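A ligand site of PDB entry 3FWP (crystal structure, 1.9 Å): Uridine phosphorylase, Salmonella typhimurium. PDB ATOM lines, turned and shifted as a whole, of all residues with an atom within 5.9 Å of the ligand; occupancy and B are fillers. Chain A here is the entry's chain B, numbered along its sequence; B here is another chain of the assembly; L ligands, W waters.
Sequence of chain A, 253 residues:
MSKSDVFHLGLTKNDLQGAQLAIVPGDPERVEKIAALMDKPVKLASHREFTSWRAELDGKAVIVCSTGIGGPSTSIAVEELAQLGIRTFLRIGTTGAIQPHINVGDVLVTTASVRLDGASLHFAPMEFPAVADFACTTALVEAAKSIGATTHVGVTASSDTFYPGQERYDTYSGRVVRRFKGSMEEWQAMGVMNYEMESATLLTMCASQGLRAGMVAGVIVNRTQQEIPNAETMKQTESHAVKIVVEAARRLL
OE2 of Glu 198 lies within hydrogen-bond range of O1 of the ligand, 2.4 Å away. A ring nitrogen (NE2) of His 8 of chain B sits at hydrogen-bond distance from an oxygen (O5) of the ligand (2.7 Å). The guanidinium group of Arg 168 sits at hydrogen-bond distance from an oxygen (O3) of the ligand (2.8 Å). OG1 of Thr 94 lies within hydrogen-bond range of O4 of the ligand (3.0 Å). OE1 of Gln 166 sits close to O3 of the ligand.
Water W2 lies within hydrogen-bond range of OE1 of Gln 166 (2.6 Å), O3 of the ligand (2.6 Å), NH1 of Arg 223 (3.1 Å) and NH2 of Arg 168 (3.2 Å). Water W1 bridges O5 of the ligand and NH2 of Arg 48 of chain B.
The side-chain sulfur (SD) of Met 197 sits close to an oxygen (O2) of the ligand. Residues that only touch the ligand: Ile 69 (3.6 Å), Thr 95 (3.6 Å), Gly 96 (3.6 Å), Phe 162 (3.4 Å), Glu 196 (3.6 Å), Ile 220 (3.8 Å), Phe 7 of chain B (3.9 Å) and Arg 48 of chain B (3.5 Å). Hydrophobic or aromatic side chains within 4 Å of the ligand: Ile 69, Phe 162, Met 197, Ile 220, Phe 7 of chain B and His 8 of chain B. The nearest printed residue that does not touch the ligand is Tyr 195 (4.1 Å).
The guanidinium group (NH2) of Arg 91 is in salt-bridge range of the side-chain carboxylate (OE1) of Glu 198, 3.0 Å away. The side-chain carboxylate of Glu 198 sits at hydrogen-bond distance from the backbone NH of Gly 70, at 2.7 Å. O of Gln 166 is in hydrogen-bond range of NH1 of Arg 223 (2.7 Å). The backbone NH (N) of Phe 162 lies close to the side-chain sulfur (SD) of Met 197, 3.7 Å away. The backbone carbonyl oxygen (O) of Thr 95 sits at hydrogen-bond distance from the backbone NH (N) of Ile 220 (2.9 Å). The side-chain hydroxyl (OG1) of Thr 95 lies within hydrogen-bond range of the backbone carbonyl oxygen (O) of Tyr 195 (2.5 Å). N of Tyr 195 lies within hydrogen-bond range of O of Gly 96 (2.8 Å). NE of Arg 91 lies within salt-bridge range of OE1 of Glu 196 (3.0 Å).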
ATOM      1  N   GLY A  26     -22.829  12.420  18.336  1.00  0.00           N
ATOM      2  CA  GLY A  26     -21.866  13.485  18.087  1.00  0.00           C
ATOM      3  C   GLY A  26     -22.517  14.852  18.128  1.00  0.00           C
ATOM      4  O   GLY A  26     -22.003  15.786  18.731  1.00  0.00           O
ATOM      5  N   GLY A  68     -19.701  16.040  20.578  1.00  0.00           N
ATOM      6  CA  GLY A  68     -19.122  16.890  19.564  1.00  0.00           C
ATOM      7  C   GLY A  68     -18.413  16.039  18.525  1.00  0.00           C
ATOM      8  O   GLY A  68     -18.350  14.812  18.664  1.00  0.00           O
ATOM      9  N   ILE A  69     -17.856  16.669  17.503  1.00  0.00           N
ATOM     10  CA  ILE A  69     -17.072  15.954  16.490  1.00  0.00           C
ATOM     11  C   ILE A  69     -15.650  15.698  16.983  1.00  0.00           C
ATOM     12  O   ILE A  69     -14.974  16.616  17.459  1.00  0.00           O
ATOM     13  CB  ILE A  69     -17.025  16.746  15.162  1.00  0.00           C
ATOM     14  CG1 ILE A  69     -18.420  16.801  14.525  1.00  0.00           C
ATOM     15  CG2 ILE A  69     -16.008  16.124  14.203  1.00  0.00           C
ATOM     16  CD1 ILE A  69     -18.530  17.749  13.359  1.00  0.00           C
ATOM     17  N   GLY A  70     -15.202  14.447  16.894  1.00  0.00           N
ATOM     18  CA  GLY A  70     -13.808  14.133  17.065  1.00  0.00           C
ATOM     19  C   GLY A  70     -13.426  13.528  18.406  1.00  0.00           C
ATOM     20  O   GLY A  70     -14.119  13.713  19.419  1.00  0.00           O
ATOM     21  N   ARG A  91     -22.177   4.785  21.364  1.00  0.00           N
ATOM     22  CA  ARG A  91     -22.110   5.850  20.373  1.00  0.00           C
ATOM     23  C   ARG A  91     -23.102   5.575  19.250  1.00  0.00           C
ATOM     24  O   ARG A  91     -23.182   4.477  18.724  1.00  0.00           O
ATOM     25  CB  ARG A  91     -20.705   6.036  19.806  1.00  0.00           C
ATOM     26  CG  ARG A  91     -20.682   7.116  18.724  1.00  0.00           C
ATOM     27  CD  ARG A  91     -19.273   7.578  18.323  1.00  0.00           C
ATOM     28  NE  ARG A  91     -19.196   7.759  16.867  1.00  0.00           N
ATOM     29  CZ  ARG A  91     -19.788   8.736  16.184  1.00  0.00           C
ATOM     30  NH1 ARG A  91     -20.500   9.672  16.818  1.00  0.00           N
ATOM     31  NH2 ARG A  91     -19.664   8.786  14.869  1.00  0.00           N
ATOM     32  N   GLY A  93     -23.858   7.374  15.687  1.00  0.00           N
ATOM     33  CA  GLY A  93     -23.284   8.362  14.783  1.00  0.00           C
ATOM     34  C   GLY A  93     -23.870   8.357  13.387  1.00  0.00           C
ATOM     35  O   GLY A  93     -24.825   7.638  13.100  1.00  0.00           O
ATOM     36  N   THR A  94     -23.296   9.209  12.540  1.00  0.00           N
ATOM     37  CA  THR A  94     -23.525   9.195  11.102  1.00  0.00           C
ATOM     38  C   THR A  94     -22.201   8.821  10.432  1.00  0.00           C
ATOM     39  O   THR A  94     -21.126   8.977  11.031  1.00  0.00           O
ATOM     40  CB  THR A  94     -24.044  10.558  10.567  1.00  0.00           C
ATOM     41  OG1 THR A  94     -23.114  11.607  10.886  1.00  0.00           O
ATOM     42  CG2 THR A  94     -25.411  10.894  11.150  1.00  0.00           C
ATOM     43  N   THR A  95     -22.272   8.313   9.209  1.00  0.00           N
ATOM     44  CA  THR A  95     -21.098   7.699   8.615  1.00  0.00           C
ATOM     45  C   THR A  95     -21.107   7.697   7.089  1.00  0.00           C
ATOM     46  O   THR A  95     -22.171   7.653   6.459  1.00  0.00           O
ATOM     47  CB  THR A  95     -20.891   6.247   9.149  1.00  0.00           C
ATOM     48  OG1 THR A  95     -19.604   5.762   8.758  1.00  0.00           O
ATOM     49  CG2 THR A  95     -21.962   5.287   8.648  1.00  0.00           C
ATOM     50  N   GLY A  96     -19.909   7.752   6.511  1.00  0.00           N
ATOM     51  CA  GLY A  96     -19.726   7.551   5.089  1.00  0.00           C
ATOM     52  C   GLY A  96     -19.295   6.120   4.797  1.00  0.00           C
ATOM     53  O   GLY A  96     -18.250   5.676   5.275  1.00  0.00           O
ATOM     54  N   PHE A 162     -12.263  15.138   8.683  1.00  0.00           N
ATOM     55  CA  PHE A 162     -13.358  14.851   7.763  1.00  0.00           C
ATOM     56  C   PHE A 162     -12.822  14.793   6.338  1.00  0.00           C
ATOM     57  O   PHE A 162     -13.310  14.021   5.496  1.00  0.00           O
ATOM     58  CB  PHE A 162     -14.429  15.941   7.884  1.00  0.00           C
ATOM     59  CG  PHE A 162     -15.668  15.688   7.068  1.00  0.00           C
ATOM     60  CD1 PHE A 162     -15.835  16.294   5.817  1.00  0.00           C
ATOM     61  CD2 PHE A 162     -16.680  14.854   7.553  1.00  0.00           C
ATOM     62  CE1 PHE A 162     -16.996  16.073   5.068  1.00  0.00           C
ATOM     63  CE2 PHE A 162     -17.839  14.631   6.813  1.00  0.00           C
ATOM     64  CZ  PHE A 162     -18.005  15.238   5.562  1.00  0.00           C
ATOM     65  N   GLN A 166      -9.947  11.177   5.381  1.00  0.00           N
ATOM     66  CA  GLN A 166     -10.953  10.324   4.740  1.00  0.00           C
ATOM     67  C   GLN A 166     -10.790  10.378   3.227  1.00  0.00           C
ATOM     68  O   GLN A 166     -11.686  10.001   2.474  1.00  0.00           O
ATOM     69  CB  GLN A 166     -12.369  10.730   5.177  1.00  0.00           C
ATOM     70  CG  GLN A 166     -12.588  10.657   6.692  1.00  0.00           C
ATOM     71  CD  GLN A 166     -14.035  10.826   7.100  1.00  0.00           C
ATOM     72  OE1 GLN A 166     -14.953  10.472   6.366  1.00  0.00           O
ATOM     73  NE2 GLN A 166     -14.251  11.374   8.288  1.00  0.00           N
ATOM     74  N   ARG A 168     -10.806  12.836   1.060  1.00  0.00           N
ATOM     75  CA  ARG A 168     -11.643  13.737   0.266  1.00  0.00           C
ATOM     76  C   ARG A 168     -10.742  14.748  -0.430  1.00  0.00           C
ATOM     77  O   ARG A 168      -9.863  15.341   0.196  1.00  0.00           O
ATOM     78  CB  ARG A 168     -12.664  14.445   1.153  1.00  0.00           C
ATOM     79  CG  ARG A 168     -13.809  13.569   1.605  1.00  0.00           C
ATOM     80  CD  ARG A 168     -14.764  14.346   2.493  1.00  0.00           C
ATOM     81  NE  ARG A 168     -16.047  13.659   2.628  1.00  0.00           N
ATOM     82  CZ  ARG A 168     -16.428  12.920   3.676  1.00  0.00           C
ATOM     83  NH1 ARG A 168     -15.621  12.767   4.726  1.00  0.00           N
ATOM     84  NH2 ARG A 168     -17.624  12.356   3.667  1.00  0.00           N
ATOM     85  N   TYR A 195     -16.273   5.244   7.214  1.00  0.00           N
ATOM     86  CA  TYR A 195     -15.518   6.268   7.899  1.00  0.00           C
ATOM     87  C   TYR A 195     -16.402   6.962   8.904  1.00  0.00           C
ATOM     88  O   TYR A 195     -17.559   7.266   8.607  1.00  0.00           O
ATOM     89  CB  TYR A 195     -15.081   7.359   6.928  1.00  0.00           C
ATOM     90  CG  TYR A 195     -13.853   7.116   6.091  1.00  0.00           C
ATOM     91  CD1 TYR A 195     -12.618   6.841   6.683  1.00  0.00           C
ATOM     92  CD2 TYR A 195     -13.916   7.239   4.707  1.00  0.00           C
ATOM     93  CE1 TYR A 195     -11.480   6.665   5.897  1.00  0.00           C
ATOM     94  CE2 TYR A 195     -12.789   7.066   3.914  1.00  0.00           C
ATOM     95  CZ  TYR A 195     -11.577   6.775   4.510  1.00  0.00           C
ATOM     96  OH  TYR A 195     -10.462   6.593   3.720  1.00  0.00           O
ATOM     97  N   GLU A 196     -15.851   7.232  10.079  1.00  0.00           N
ATOM     98  CA  GLU A 196     -16.357   8.298  10.943  1.00  0.00           C
ATOM     99  C   GLU A 196     -15.181   8.882  11.729  1.00  0.00           C
ATOM    100  O   GLU A 196     -14.028   8.712  11.325  1.00  0.00           O
ATOM    101  CB  GLU A 196     -17.568   7.861  11.805  1.00  0.00           C
ATOM    102  CG  GLU A 196     -17.414   6.559  12.577  1.00  0.00           C
ATOM    103  CD  GLU A 196     -16.537   6.720  13.779  1.00  0.00           C
ATOM    104  OE1 GLU A 196     -17.022   7.271  14.798  1.00  0.00           O
ATOM    105  OE2 GLU A 196     -15.360   6.331  13.718  1.00  0.00           O
ATOM    106  N   MET A 197     -15.444   9.588  12.832  1.00  0.00           N
ATOM    107  CA  MET A 197     -14.393  10.371  13.454  1.00  0.00           C
ATOM    108  C   MET A 197     -14.207  10.205  14.968  1.00  0.00           C
ATOM    109  O   MET A 197     -13.355  10.866  15.566  1.00  0.00           O
ATOM    110  CB  MET A 197     -14.582  11.860  13.107  1.00  0.00           C
ATOM    111  CG  MET A 197     -14.409  12.156  11.619  1.00  0.00           C
ATOM    112  SD  MET A 197     -14.724  13.879  11.195  1.00  0.00           S
ATOM    113  CE  MET A 197     -13.404  14.695  12.073  1.00  0.00           C
ATOM    114  N   GLU A 198     -14.991   9.317  15.584  1.00  0.00           N
ATOM    115  CA  GLU A 198     -15.031   9.251  17.054  1.00  0.00           C
ATOM    116  C   GLU A 198     -14.754   7.882  17.671  1.00  0.00           C
ATOM    117  O   GLU A 198     -14.305   7.806  18.824  1.00  0.00           O
ATOM    118  CB  GLU A 198     -16.380   9.782  17.570  1.00  0.00           C
ATOM    119  CG  GLU A 198     -16.611  11.295  17.320  1.00  0.00           C
ATOM    120  CD  GLU A 198     -17.015  11.633  15.893  1.00  0.00           C
ATOM    121  OE1 GLU A 198     -17.450  10.732  15.138  1.00  0.00           O
ATOM    122  OE2 GLU A 198     -16.903  12.818  15.506  1.00  0.00           O
ATOM    123  N   ILE A 220     -24.900   8.077   5.713  1.00  0.00           N
ATOM    124  CA  ILE A 220     -25.438   9.314   5.118  1.00  0.00           C
ATOM    125  C   ILE A 220     -24.828   9.627   3.745  1.00  0.00           C
ATOM    126  O   ILE A 220     -25.310  10.512   3.023  1.00  0.00           O
ATOM    127  CB  ILE A 220     -25.299  10.539   6.070  1.00  0.00           C
ATOM    128  CG1 ILE A 220     -23.823  10.890   6.314  1.00  0.00           C
ATOM    129  CG2 ILE A 220     -26.058  10.271   7.372  1.00  0.00           C
ATOM    130  CD1 ILE A 220     -23.603  12.295   6.870  1.00  0.00           C
ATOM    131  N   VAL A 221     -23.767   8.900   3.387  1.00  0.00           N
ATOM    132  CA  VAL A 221     -23.128   9.039   2.080  1.00  0.00           C
ATOM    133  C   VAL A 221     -22.357   7.768   1.727  1.00  0.00           C
ATOM    134  O   VAL A 221     -21.778   7.109   2.605  1.00  0.00           O
ATOM    135  CB  VAL A 221     -22.201  10.305   2.019  1.00  0.00           C
ATOM    136  CG1 VAL A 221     -20.996  10.190   2.959  1.00  0.00           C
ATOM    137  CG2 VAL A 221     -21.759  10.604   0.585  1.00  0.00           C
ATOM    138  N   ARG A 223     -19.157   6.720  -0.267  1.00  0.00           N
ATOM    139  CA  ARG A 223     -17.937   7.339  -0.768  1.00  0.00           C
ATOM    140  C   ARG A 223     -17.401   6.763  -2.074  1.00  0.00           C
ATOM    141  O   ARG A 223     -16.528   7.358  -2.705  1.00  0.00           O
ATOM    142  CB  ARG A 223     -16.842   7.320   0.316  1.00  0.00           C
ATOM    143  CG  ARG A 223     -17.149   8.202   1.523  1.00  0.00           C
ATOM    144  CD  ARG A 223     -17.031   9.690   1.179  1.00  0.00           C
ATOM    145  NE  ARG A 223     -15.812  10.007   0.426  1.00  0.00           N
ATOM    146  CZ  ARG A 223     -14.595  10.055   0.965  1.00  0.00           C
ATOM    147  NH1 ARG A 223     -14.416   9.832   2.266  1.00  0.00           N
ATOM    148  NH2 ARG A 223     -13.551  10.347   0.204  1.00  0.00           N
ATOM    149  N   GLU A 227     -18.187  12.397  -2.347  1.00  0.00           N
ATOM    150  CA  GLU A 227     -17.530  12.785  -1.103  1.00  0.00           C
ATOM    151  C   GLU A 227     -18.519  13.314  -0.058  1.00  0.00           C
ATOM    152  O   GLU A 227     -18.339  13.086   1.138  1.00  0.00           O
ATOM    153  CB  GLU A 227     -16.431  13.813  -1.371  1.00  0.00           C
ATOM    154  CG  GLU A 227     -15.328  13.283  -2.270  1.00  0.00           C
ATOM    155  CD  GLU A 227     -14.121  14.196  -2.340  1.00  0.00           C
ATOM    156  OE1 GLU A 227     -14.178  15.321  -1.795  1.00  0.00           O
ATOM    157  OE2 GLU A 227     -13.100  13.788  -2.943  1.00  0.00           O
ATOM    158  N   PHE B   7     -20.461  21.839   3.973  1.00  0.00           N
ATOM    159  CA  PHE B   7     -21.216  20.761   4.592  1.00  0.00           C
ATOM    160  C   PHE B   7     -21.583  20.965   6.073  1.00  0.00           C
ATOM    161  O   PHE B   7     -22.663  20.548   6.487  1.00  0.00           O
ATOM    162  CB  PHE B   7     -20.509  19.411   4.403  1.00  0.00           C
ATOM    163  CG  PHE B   7     -21.338  18.227   4.832  1.00  0.00           C
ATOM    164  CD1 PHE B   7     -22.537  17.925   4.188  1.00  0.00           C
ATOM    165  CD2 PHE B   7     -20.923  17.427   5.893  1.00  0.00           C
ATOM    166  CE1 PHE B   7     -23.306  16.833   4.581  1.00  0.00           C
ATOM    167  CE2 PHE B   7     -21.697  16.334   6.308  1.00  0.00           C
ATOM    168  CZ  PHE B   7     -22.878  16.040   5.649  1.00  0.00           C
ATOM    169  N   HIS B   8     -20.700  21.579   6.846  1.00  0.00           N
ATOM    170  CA  HIS B   8     -20.934  21.686   8.301  1.00  0.00           C
ATOM    171  C   HIS B   8     -21.377  23.068   8.768  1.00  0.00           C
ATOM    172  O   HIS B   8     -22.305  23.170   9.563  1.00  0.00           O
ATOM    173  CB  HIS B   8     -19.695  21.257   9.083  1.00  0.00           C
ATOM    174  CG  HIS B   8     -19.324  19.823   8.879  1.00  0.00           C
ATOM    175  ND1 HIS B   8     -18.467  19.409   7.891  1.00  0.00           N
ATOM    176  CD2 HIS B   8     -19.704  18.708   9.542  1.00  0.00           C
ATOM    177  CE1 HIS B   8     -18.316  18.098   7.946  1.00  0.00           C
ATOM    178  NE2 HIS B   8     -19.072  17.643   8.936  1.00  0.00           N
ATOM    179  N   ARG B  48     -24.141  22.189  14.999  1.00  0.00           N
ATOM    180  CA  ARG B  48     -23.231  21.443  15.874  1.00  0.00           C
ATOM    181  C   ARG B  48     -22.439  22.427  16.752  1.00  0.00           C
ATOM    182  O   ARG B  48     -23.024  23.352  17.320  1.00  0.00           O
ATOM    183  CB  ARG B  48     -22.308  20.537  15.032  1.00  0.00           C
ATOM    184  CG  ARG B  48     -23.017  19.406  14.282  1.00  0.00           C
ATOM    185  CD  ARG B  48     -22.050  18.690  13.357  1.00  0.00           C
ATOM    186  NE  ARG B  48     -22.587  17.477  12.708  1.00  0.00           N
ATOM    187  CZ  ARG B  48     -22.460  16.238  13.193  1.00  0.00           C
ATOM    188  NH1 ARG B  48     -21.840  16.005  14.346  1.00  0.00           N
ATOM    189  NH2 ARG B  48     -22.972  15.216  12.507  1.00  0.00           N
ATOM    190  N   ILE B  76     -12.323  20.990  10.386  1.00  0.00           N
ATOM    191  CA  ILE B  76     -13.542  21.170   9.613  1.00  0.00           C
ATOM    192  C   ILE B  76     -13.875  22.648   9.438  1.00  0.00           C
ATOM    193  O   ILE B  76     -14.086  23.103   8.317  1.00  0.00           O
ATOM    194  CB  ILE B  76     -14.749  20.448  10.266  1.00  0.00           C
ATOM    195  CG1 ILE B  76     -14.594  18.932  10.140  1.00  0.00           C
ATOM    196  CG2 ILE B  76     -16.073  20.928   9.636  1.00  0.00           C
ATOM    197  CD1 ILE B  76     -15.648  18.132  10.900  1.00  0.00           C
HETATM  198  O1  LIG L   1     -18.604  13.269  13.860  1.00  0.00           O
HETATM  199  C1  LIG L   1     -18.538  13.069  12.469  1.00  0.00           C
HETATM  200  C2  LIG L   1     -18.629  11.768  11.964  1.00  0.00           C
HETATM  201  O2  LIG L   1     -17.585  11.713  10.988  1.00  0.00           O
HETATM  202  C3  LIG L   1     -18.176  11.517   9.738  1.00  0.00           C
HETATM  203  N1  LIG L   1     -17.639  11.319   8.442  1.00  0.00           N
HETATM  204  C4  LIG L   1     -18.484  11.163   7.389  1.00  0.00           C
HETATM  205  O3  LIG L   1     -17.948  10.964   6.093  1.00  0.00           O
HETATM  206  C5  LIG L   1     -20.016  11.197   7.586  1.00  0.00           C
HETATM  207  C6  LIG L   1     -20.538  11.402   8.889  1.00  0.00           C
HETATM  208  N2  LIG L   1     -19.703  11.560   9.946  1.00  0.00           N
HETATM  209  C7  LIG L   1     -19.940  11.752  11.183  1.00  0.00           C
HETATM  210  O4  LIG L   1     -20.492  13.065  11.276  1.00  0.00           O
HETATM  211  C8  LIG L   1     -19.477  13.891  11.631  1.00  0.00           C
HETATM  212  C9  LIG L   1     -18.916  14.848  10.592  1.00  0.00           C
HETATM  213  O5  LIG L   1     -19.791  15.129   9.512  1.00  0.00           O
HETATM  214  O   HOH W   1     -22.466  15.348   9.654  1.00  0.00           O
HETATM  215  O   HOH W   2     -16.501   9.461   4.549  1.00  0.00           O
